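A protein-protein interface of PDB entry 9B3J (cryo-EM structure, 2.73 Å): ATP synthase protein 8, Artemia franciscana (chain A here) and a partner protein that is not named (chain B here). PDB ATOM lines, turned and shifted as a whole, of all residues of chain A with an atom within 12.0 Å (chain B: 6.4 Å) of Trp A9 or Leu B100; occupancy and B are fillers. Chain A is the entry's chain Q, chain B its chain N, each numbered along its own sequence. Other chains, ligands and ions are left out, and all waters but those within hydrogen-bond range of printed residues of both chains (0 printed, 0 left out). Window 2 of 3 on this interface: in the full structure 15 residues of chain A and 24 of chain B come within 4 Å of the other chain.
Of the printed residues of chain B, Trp A9 touches Ala B97 and Leu B100. Of chain A, only Trp A9 (3.9 Å) comes within 4 Å of Leu B100. Ala B97 touches one residue of chain A. Printed residues of chain A within 4 Å of Val B98: Ser A16. Ser B101 touches three residues of chain A. Of chain A, only Ser A16 and Leu A20 come within 4 Å of Leu B102. Ala B103 touches none of the printed residues of chain A. No residue of chain A comes within 4 Å of Pro B151. No residue of chain A comes within 4 Å of Ile B152. Of the printed residues of chain B, Ser A16 touches Val B98 (3.97 Å), Ser B101 (3.6 Å) and Leu B102 (3.7 Å). Printed residues of chain B within 4 Å of Phe A13: Ser B101 (3.3 Å) and Pro B105 (3.7 Å). Of the printed residues of chain B, Leu A20 touches Leu B102. Printed residues of chain B within 4 Å of Met A17: Ser B101 (3.3 Å) and Pro B105 (3.7 Å). Of the printed residues of chain A, Pro B105 touches Phe A13 (3.7 Å) and Met A17 (3.7 Å). Leu A14 touches none of the printed residues of chain B. The nearest residue of chain B that does not touch Trp A9 is Leu B96 (4.8 Å). The nearest residue of chain A that does not touch Leu B100 is Phe A13 (5.4 Å).
Among the printed residues, merely in contact across the chains: Met A17 with Ser B101 (3.3 Å), Phe A13 with Ser B101 (3.3 Å), Ser A16 with Ser B101 (3.6 Å), Phe A13 with Pro B105 (3.7 Å), Met A17 with Pro B105 (3.7 Å), Ser A16 with Leu B102 (3.7 Å), Trp A9 with Ala B97 (3.8 Å), Leu A20 with Leu B102 (3.9 Å), Trp A9 with Leu B100 (3.9 Å) and Ser A16 with Val B98 (3.97 Å).
Of the 15 printed residues of chain B, 6 touch a printed residue of chain A. Of the 12 printed residues of chain A, 5 touch a printed residue of chain B. Printed residues of chain A that touch a printed residue of chain B: Trp A9, Phe A13, Ser A16, Met A17 and Leu A20. Hydrophobic or aromatic side chains of chain A within 4 Å of the printed part of chain B: Trp A9, Phe A13, Met A17 and Leu A20.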
ATOM      1  N   PRO A   8     -14.932 -23.358  22.559  1.00  0.00           N
ATOM      2  CA  PRO A   8     -15.329 -22.135  21.854  1.00  0.00           C
ATOM      3  C   PRO A   8     -16.273 -22.433  20.704  1.00  0.00           C
ATOM      4  O   PRO A   8     -16.058 -21.939  19.599  1.00  0.00           O
ATOM      5  CB  PRO A   8     -13.999 -21.590  21.337  1.00  0.00           C
ATOM      6  CG  PRO A   8     -13.180 -22.810  21.110  1.00  0.00           C
ATOM      7  CD  PRO A   8     -13.573 -23.788  22.188  1.00  0.00           C
ATOM      8  N   TRP A   9     -17.306 -23.234  20.972  1.00  0.00           N
ATOM      9  CA  TRP A   9     -18.188 -23.701  19.909  1.00  0.00           C
ATOM     10  C   TRP A   9     -18.994 -22.568  19.293  1.00  0.00           C
ATOM     11  O   TRP A   9     -19.372 -22.652  18.122  1.00  0.00           O
ATOM     12  CB  TRP A   9     -19.134 -24.772  20.440  1.00  0.00           C
ATOM     13  CG  TRP A   9     -18.481 -26.065  20.792  1.00  0.00           C
ATOM     14  CD1 TRP A   9     -17.490 -26.266  21.705  1.00  0.00           C
ATOM     15  CD2 TRP A   9     -18.804 -27.352  20.262  1.00  0.00           C
ATOM     16  NE1 TRP A   9     -17.163 -27.596  21.764  1.00  0.00           N
ATOM     17  CE2 TRP A   9     -17.958 -28.285  20.888  1.00  0.00           C
ATOM     18  CE3 TRP A   9     -19.723 -27.806  19.314  1.00  0.00           C
ATOM     19  CZ2 TRP A   9     -18.004 -29.644  20.596  1.00  0.00           C
ATOM     20  CZ3 TRP A   9     -19.766 -29.155  19.025  1.00  0.00           C
ATOM     21  CH2 TRP A   9     -18.913 -30.056  19.662  1.00  0.00           C
ATOM     22  N   ILE A  10     -19.280 -21.519  20.061  1.00  0.00           N
ATOM     23  CA  ILE A  10     -20.048 -20.395  19.532  1.00  0.00           C
ATOM     24  C   ILE A  10     -19.226 -19.619  18.510  1.00  0.00           C
ATOM     25  O   ILE A  10     -19.712 -19.282  17.421  1.00  0.00           O
ATOM     26  CB  ILE A  10     -20.523 -19.490  20.682  1.00  0.00           C
ATOM     27  CG1 ILE A  10     -21.493 -20.246  21.588  1.00  0.00           C
ATOM     28  CG2 ILE A  10     -21.175 -18.227  20.142  1.00  0.00           C
ATOM     29  CD1 ILE A  10     -21.937 -19.443  22.791  1.00  0.00           C
ATOM     30  N   MET A  11     -17.967 -19.327  18.838  1.00  0.00           N
ATOM     31  CA  MET A  11     -17.113 -18.629  17.886  1.00  0.00           C
ATOM     32  C   MET A  11     -16.764 -19.513  16.700  1.00  0.00           C
ATOM     33  O   MET A  11     -16.618 -19.009  15.582  1.00  0.00           O
ATOM     34  CB  MET A  11     -15.843 -18.132  18.569  1.00  0.00           C
ATOM     35  CG  MET A  11     -16.061 -16.944  19.485  1.00  0.00           C
ATOM     36  SD  MET A  11     -14.531 -16.363  20.238  1.00  0.00           S
ATOM     37  CE  MET A  11     -15.129 -14.976  21.197  1.00  0.00           C
ATOM     38  N   VAL A  12     -16.643 -20.824  16.920  1.00  0.00           N
ATOM     39  CA  VAL A  12     -16.430 -21.748  15.809  1.00  0.00           C
ATOM     40  C   VAL A  12     -17.630 -21.739  14.872  1.00  0.00           C
ATOM     41  O   VAL A  12     -17.474 -21.662  13.650  1.00  0.00           O
ATOM     42  CB  VAL A  12     -16.126 -23.161  16.341  1.00  0.00           C
ATOM     43  CG1 VAL A  12     -16.378 -24.211  15.281  1.00  0.00           C
ATOM     44  CG2 VAL A  12     -14.692 -23.233  16.802  1.00  0.00           C
ATOM     45  N   PHE A  13     -18.842 -21.775  15.431  1.00  0.00           N
ATOM     46  CA  PHE A  13     -20.057 -21.755  14.620  1.00  0.00           C
ATOM     47  C   PHE A  13     -20.182 -20.459  13.830  1.00  0.00           C
ATOM     48  O   PHE A  13     -20.523 -20.478  12.639  1.00  0.00           O
ATOM     49  CB  PHE A  13     -21.275 -21.950  15.522  1.00  0.00           C
ATOM     50  CG  PHE A  13     -22.563 -22.145  14.779  1.00  0.00           C
ATOM     51  CD1 PHE A  13     -22.989 -23.413  14.442  1.00  0.00           C
ATOM     52  CD2 PHE A  13     -23.363 -21.066  14.447  1.00  0.00           C
ATOM     53  CE1 PHE A  13     -24.175 -23.599  13.770  1.00  0.00           C
ATOM     54  CE2 PHE A  13     -24.546 -21.247  13.773  1.00  0.00           C
ATOM     55  CZ  PHE A  13     -24.952 -22.513  13.435  1.00  0.00           C
ATOM     56  N   LEU A  14     -19.899 -19.325  14.469  1.00  0.00           N
ATOM     57  CA  LEU A  14     -20.046 -18.048  13.777  1.00  0.00           C
ATOM     58  C   LEU A  14     -18.992 -17.876  12.688  1.00  0.00           C
ATOM     59  O   LEU A  14     -19.302 -17.389  11.593  1.00  0.00           O
ATOM     60  CB  LEU A  14     -19.979 -16.897  14.777  1.00  0.00           C
ATOM     61  CG  LEU A  14     -20.025 -15.487  14.188  1.00  0.00           C
ATOM     62  CD1 LEU A  14     -21.343 -15.260  13.471  1.00  0.00           C
ATOM     63  CD2 LEU A  14     -19.803 -14.440  15.268  1.00  0.00           C
ATOM     64  N   VAL A  15     -17.749 -18.280  12.959  1.00  0.00           N
ATOM     65  CA  VAL A  15     -16.698 -18.143  11.959  1.00  0.00           C
ATOM     66  C   VAL A  15     -16.908 -19.126  10.812  1.00  0.00           C
ATOM     67  O   VAL A  15     -16.698 -18.784   9.642  1.00  0.00           O
ATOM     68  CB  VAL A  15     -15.319 -18.300  12.624  1.00  0.00           C
ATOM     69  CG1 VAL A  15     -14.219 -18.447  11.590  1.00  0.00           C
ATOM     70  CG2 VAL A  15     -15.034 -17.095  13.489  1.00  0.00           C
ATOM     71  N   SER A  16     -17.356 -20.348  11.115  1.00  0.00           N
ATOM     72  CA  SER A  16     -17.603 -21.322  10.061  1.00  0.00           C
ATOM     73  C   SER A  16     -18.732 -20.877   9.147  1.00  0.00           C
ATOM     74  O   SER A  16     -18.639 -21.025   7.925  1.00  0.00           O
ATOM     75  CB  SER A  16     -17.918 -22.685  10.662  1.00  0.00           C
ATOM     76  OG  SER A  16     -18.326 -23.587   9.654  1.00  0.00           O
ATOM     77  N   MET A  17     -19.800 -20.305   9.712  1.00  0.00           N
ATOM     78  CA  MET A  17     -20.907 -19.866   8.867  1.00  0.00           C
ATOM     79  C   MET A  17     -20.573 -18.598   8.099  1.00  0.00           C
ATOM     80  O   MET A  17     -21.031 -18.430   6.963  1.00  0.00           O
ATOM     81  CB  MET A  17     -22.163 -19.658   9.701  1.00  0.00           C
ATOM     82  CG  MET A  17     -22.907 -20.935   9.966  1.00  0.00           C
ATOM     83  SD  MET A  17     -22.851 -21.996   8.520  1.00  0.00           S
ATOM     84  CE  MET A  17     -24.193 -23.111   8.889  1.00  0.00           C
ATOM     85  N   ALA A  18     -19.784 -17.698   8.687  1.00  0.00           N
ATOM     86  CA  ALA A  18     -19.344 -16.524   7.945  1.00  0.00           C
ATOM     87  C   ALA A  18     -18.437 -16.916   6.795  1.00  0.00           C
ATOM     88  O   ALA A  18     -18.483 -16.308   5.723  1.00  0.00           O
ATOM     89  CB  ALA A  18     -18.627 -15.554   8.875  1.00  0.00           C
ATOM     90  N   LEU A  20     -18.563 -19.921   5.252  1.00  0.00           N
ATOM     91  CA  LEU A  20     -19.397 -20.602   4.270  1.00  0.00           C
ATOM     92  C   LEU A  20     -20.187 -19.607   3.437  1.00  0.00           C
ATOM     93  O   LEU A  20     -20.373 -19.806   2.231  1.00  0.00           O
ATOM     94  CB  LEU A  20     -20.333 -21.577   4.965  1.00  0.00           C
ATOM     95  CG  LEU A  20     -21.207 -22.422   4.052  1.00  0.00           C
ATOM     96  CD1 LEU A  20     -20.346 -23.160   3.074  1.00  0.00           C
ATOM     97  CD2 LEU A  20     -21.996 -23.391   4.885  1.00  0.00           C
ATOM     98  N   HIS B  95     -12.250 -31.875  13.459  1.00  0.00           N
ATOM     99  CA  HIS B  95     -13.031 -31.710  14.675  1.00  0.00           C
ATOM    100  C   HIS B  95     -14.515 -31.869  14.392  1.00  0.00           C
ATOM    101  O   HIS B  95     -15.008 -31.450  13.344  1.00  0.00           O
ATOM    102  CB  HIS B  95     -12.763 -30.344  15.292  1.00  0.00           C
ATOM    103  CG  HIS B  95     -11.415 -30.233  15.923  1.00  0.00           C
ATOM    104  ND1 HIS B  95     -11.242 -30.076  17.279  1.00  0.00           N
ATOM    105  CD2 HIS B  95     -10.175 -30.281  15.386  1.00  0.00           C
ATOM    106  CE1 HIS B  95      -9.951 -30.018  17.549  1.00  0.00           C
ATOM    107  NE2 HIS B  95      -9.282 -30.141  16.418  1.00  0.00           N
ATOM    108  N   LEU B  96     -15.232 -32.470  15.345  1.00  0.00           N
ATOM    109  CA  LEU B  96     -16.667 -32.669  15.183  1.00  0.00           C
ATOM    110  C   LEU B  96     -17.449 -31.373  15.275  1.00  0.00           C
ATOM    111  O   LEU B  96     -18.612 -31.343  14.861  1.00  0.00           O
ATOM    112  CB  LEU B  96     -17.210 -33.641  16.227  1.00  0.00           C
ATOM    113  CG  LEU B  96     -16.768 -35.103  16.173  1.00  0.00           C
ATOM    114  CD1 LEU B  96     -15.581 -35.353  17.094  1.00  0.00           C
ATOM    115  CD2 LEU B  96     -17.927 -36.015  16.530  1.00  0.00           C
ATOM    116  N   ALA B  97     -16.848 -30.309  15.811  1.00  0.00           N
ATOM    117  CA  ALA B  97     -17.567 -29.050  15.962  1.00  0.00           C
ATOM    118  C   ALA B  97     -17.839 -28.397  14.615  1.00  0.00           C
ATOM    119  O   ALA B  97     -18.946 -27.907  14.373  1.00  0.00           O
ATOM    120  CB  ALA B  97     -16.785 -28.101  16.865  1.00  0.00           C
ATOM    121  N   VAL B  98     -16.850 -28.389  13.722  1.00  0.00           N
ATOM    122  CA  VAL B  98     -17.028 -27.729  12.433  1.00  0.00           C
ATOM    123  C   VAL B  98     -17.976 -28.518  11.539  1.00  0.00           C
ATOM    124  O   VAL B  98     -18.837 -27.940  10.862  1.00  0.00           O
ATOM    125  CB  VAL B  98     -15.665 -27.511  11.762  1.00  0.00           C
ATOM    126  CG1 VAL B  98     -15.784 -26.464  10.678  1.00  0.00           C
ATOM    127  CG2 VAL B  98     -14.648 -27.102  12.798  1.00  0.00           C
ATOM    128  N   THR B  99     -17.840 -29.843  11.519  1.00  0.00           N
ATOM    129  CA  THR B  99     -18.738 -30.665  10.713  1.00  0.00           C
ATOM    130  C   THR B  99     -20.169 -30.604  11.237  1.00  0.00           C
ATOM    131  O   THR B  99     -21.123 -30.589  10.448  1.00  0.00           O
ATOM    132  CB  THR B  99     -18.244 -32.105  10.683  1.00  0.00           C
ATOM    133  OG1 THR B  99     -18.385 -32.681  11.982  1.00  0.00           O
ATOM    134  CG2 THR B  99     -16.792 -32.143  10.298  1.00  0.00           C
ATOM    135  N   LEU B 100     -20.338 -30.570  12.564  1.00  0.00           N
ATOM    136  CA  LEU B 100     -21.665 -30.371  13.139  1.00  0.00           C
ATOM    137  C   LEU B 100     -22.211 -28.995  12.791  1.00  0.00           C
ATOM    138  O   LEU B 100     -23.408 -28.845  12.510  1.00  0.00           O
ATOM    139  CB  LEU B 100     -21.607 -30.551  14.652  1.00  0.00           C
ATOM    140  CG  LEU B 100     -22.841 -31.017  15.410  1.00  0.00           C
ATOM    141  CD1 LEU B 100     -23.183 -32.432  15.021  1.00  0.00           C
ATOM    142  CD2 LEU B 100     -22.572 -30.921  16.896  1.00  0.00           C
ATOM    143  N   SER B 101     -21.343 -27.981  12.790  1.00  0.00           N
ATOM    144  CA  SER B 101     -21.750 -26.638  12.412  1.00  0.00           C
ATOM    145  C   SER B 101     -22.173 -26.551  10.958  1.00  0.00           C
ATOM    146  O   SER B 101     -22.932 -25.647  10.602  1.00  0.00           O
ATOM    147  CB  SER B 101     -20.611 -25.657  12.672  1.00  0.00           C
ATOM    148  OG  SER B 101     -20.875 -24.416  12.051  1.00  0.00           O
ATOM    149  N   LEU B 102     -21.680 -27.447  10.108  1.00  0.00           N
ATOM    150  CA  LEU B 102     -22.105 -27.458   8.713  1.00  0.00           C
ATOM    151  C   LEU B 102     -23.357 -28.293   8.485  1.00  0.00           C
ATOM    152  O   LEU B 102     -24.193 -27.936   7.650  1.00  0.00           O
ATOM    153  CB  LEU B 102     -20.980 -27.981   7.822  1.00  0.00           C
ATOM    154  CG  LEU B 102     -19.707 -27.142   7.786  1.00  0.00           C
ATOM    155  CD1 LEU B 102     -18.658 -27.846   6.965  1.00  0.00           C
ATOM    156  CD2 LEU B 102     -20.003 -25.773   7.225  1.00  0.00           C
ATOM    157  N   ALA B 103     -23.501 -29.400   9.213  1.00  0.00           N
ATOM    158  CA  ALA B 103     -24.565 -30.360   8.947  1.00  0.00           C
ATOM    159  C   ALA B 103     -25.871 -30.034   9.655  1.00  0.00           C
ATOM    160  O   ALA B 103     -26.943 -30.204   9.064  1.00  0.00           O
ATOM    161  CB  ALA B 103     -24.117 -31.764   9.348  1.00  0.00           C
ATOM    162  N   VAL B 104     -25.808 -29.603  10.921  1.00  0.00           N
ATOM    163  CA  VAL B 104     -27.036 -29.378  11.689  1.00  0.00           C
ATOM    164  C   VAL B 104     -27.915 -28.259  11.130  1.00  0.00           C
ATOM    165  O   VAL B 104     -29.123 -28.491  10.957  1.00  0.00           O
ATOM    166  CB  VAL B 104     -26.698 -29.187  13.178  1.00  0.00           C
ATOM    167  CG1 VAL B 104     -27.937 -28.824  13.963  1.00  0.00           C
ATOM    168  CG2 VAL B 104     -26.096 -30.449  13.734  1.00  0.00           C
ATOM    169  N   PRO B 105     -27.406 -27.039  10.842  1.00  0.00           N
ATOM    170  CA  PRO B 105     -28.330 -25.970  10.414  1.00  0.00           C
ATOM    171  C   PRO B 105     -29.053 -26.236   9.105  1.00  0.00           C
ATOM    172  O   PRO B 105     -30.236 -25.902   8.981  1.00  0.00           O
ATOM    173  CB  PRO B 105     -27.412 -24.747  10.298  1.00  0.00           C
ATOM    174  CG  PRO B 105     -26.295 -25.044  11.173  1.00  0.00           C
ATOM    175  CD  PRO B 105     -26.045 -26.485  10.976  1.00  0.00           C
ATOM    176  N   PRO B 151     -28.110 -35.503  10.666  1.00  0.00           N
ATOM    177  CA  PRO B 151     -26.937 -34.629  10.818  1.00  0.00           C
ATOM    178  C   PRO B 151     -25.840 -35.223  11.679  1.00  0.00           C
ATOM    179  O   PRO B 151     -24.674 -34.805  11.558  1.00  0.00           O
ATOM    180  CB  PRO B 151     -27.520 -33.370  11.456  1.00  0.00           C
ATOM    181  CG  PRO B 151     -28.581 -33.887  12.302  1.00  0.00           C
ATOM    182  CD  PRO B 151     -29.215 -35.002  11.515  1.00  0.00           C
ATOM    183  N   ILE B 152     -26.158 -36.206  12.520  1.00  0.00           N
ATOM    184  CA  ILE B 152     -25.105 -36.906  13.240  1.00  0.00           C
ATOM    185  C   ILE B 152     -24.294 -37.762  12.280  1.00  0.00           C
ATOM    186  O   ILE B 152     -23.061 -37.787  12.341  1.00  0.00           O
ATOM    187  CB  ILE B 152     -25.698 -37.736  14.388  1.00  0.00           C
ATOM    188  CG1 ILE B 152     -26.450 -36.822  15.351  1.00  0.00           C
ATOM    189  CG2 ILE B 152     -24.607 -38.475  15.129  1.00  0.00           C
ATOM    190  CD1 ILE B 152     -27.069 -37.546  16.512  1.00  0.00           C
ATOM    191  N   SER B 155     -21.897 -35.359  10.278  1.00  0.00           N
ATOM    192  CA  SER B 155     -20.784 -34.807  11.041  1.00  0.00           C
ATOM    193  C   SER B 155     -19.797 -35.888  11.471  1.00  0.00           C
ATOM    194  O   SER B 155     -18.580 -35.678  11.417  1.00  0.00           O
ATOM    195  CB  SER B 155     -21.325 -34.064  12.252  1.00  0.00           C
ATOM    196  OG  SER B 155     -22.482 -33.336  11.895  1.00  0.00           O
ATOM    197  N   VAL B 156     -20.302 -37.040  11.916  1.00  0.00           N
ATOM    198  CA  VAL B 156     -19.431 -38.142  12.301  1.00  0.00           C
ATOM    199  C   VAL B 156     -18.679 -38.676  11.094  1.00  0.00           C
ATOM    200  O   VAL B 156     -17.464 -38.883  11.153  1.00  0.00           O
ATOM    201  CB  VAL B 156     -20.252 -39.245  12.990  1.00  0.00           C
ATOM    202  CG1 VAL B 156     -19.462 -40.541  13.073  1.00  0.00           C
ATOM    203  CG2 VAL B 156     -20.671 -38.791  14.369  1.00  0.00           C
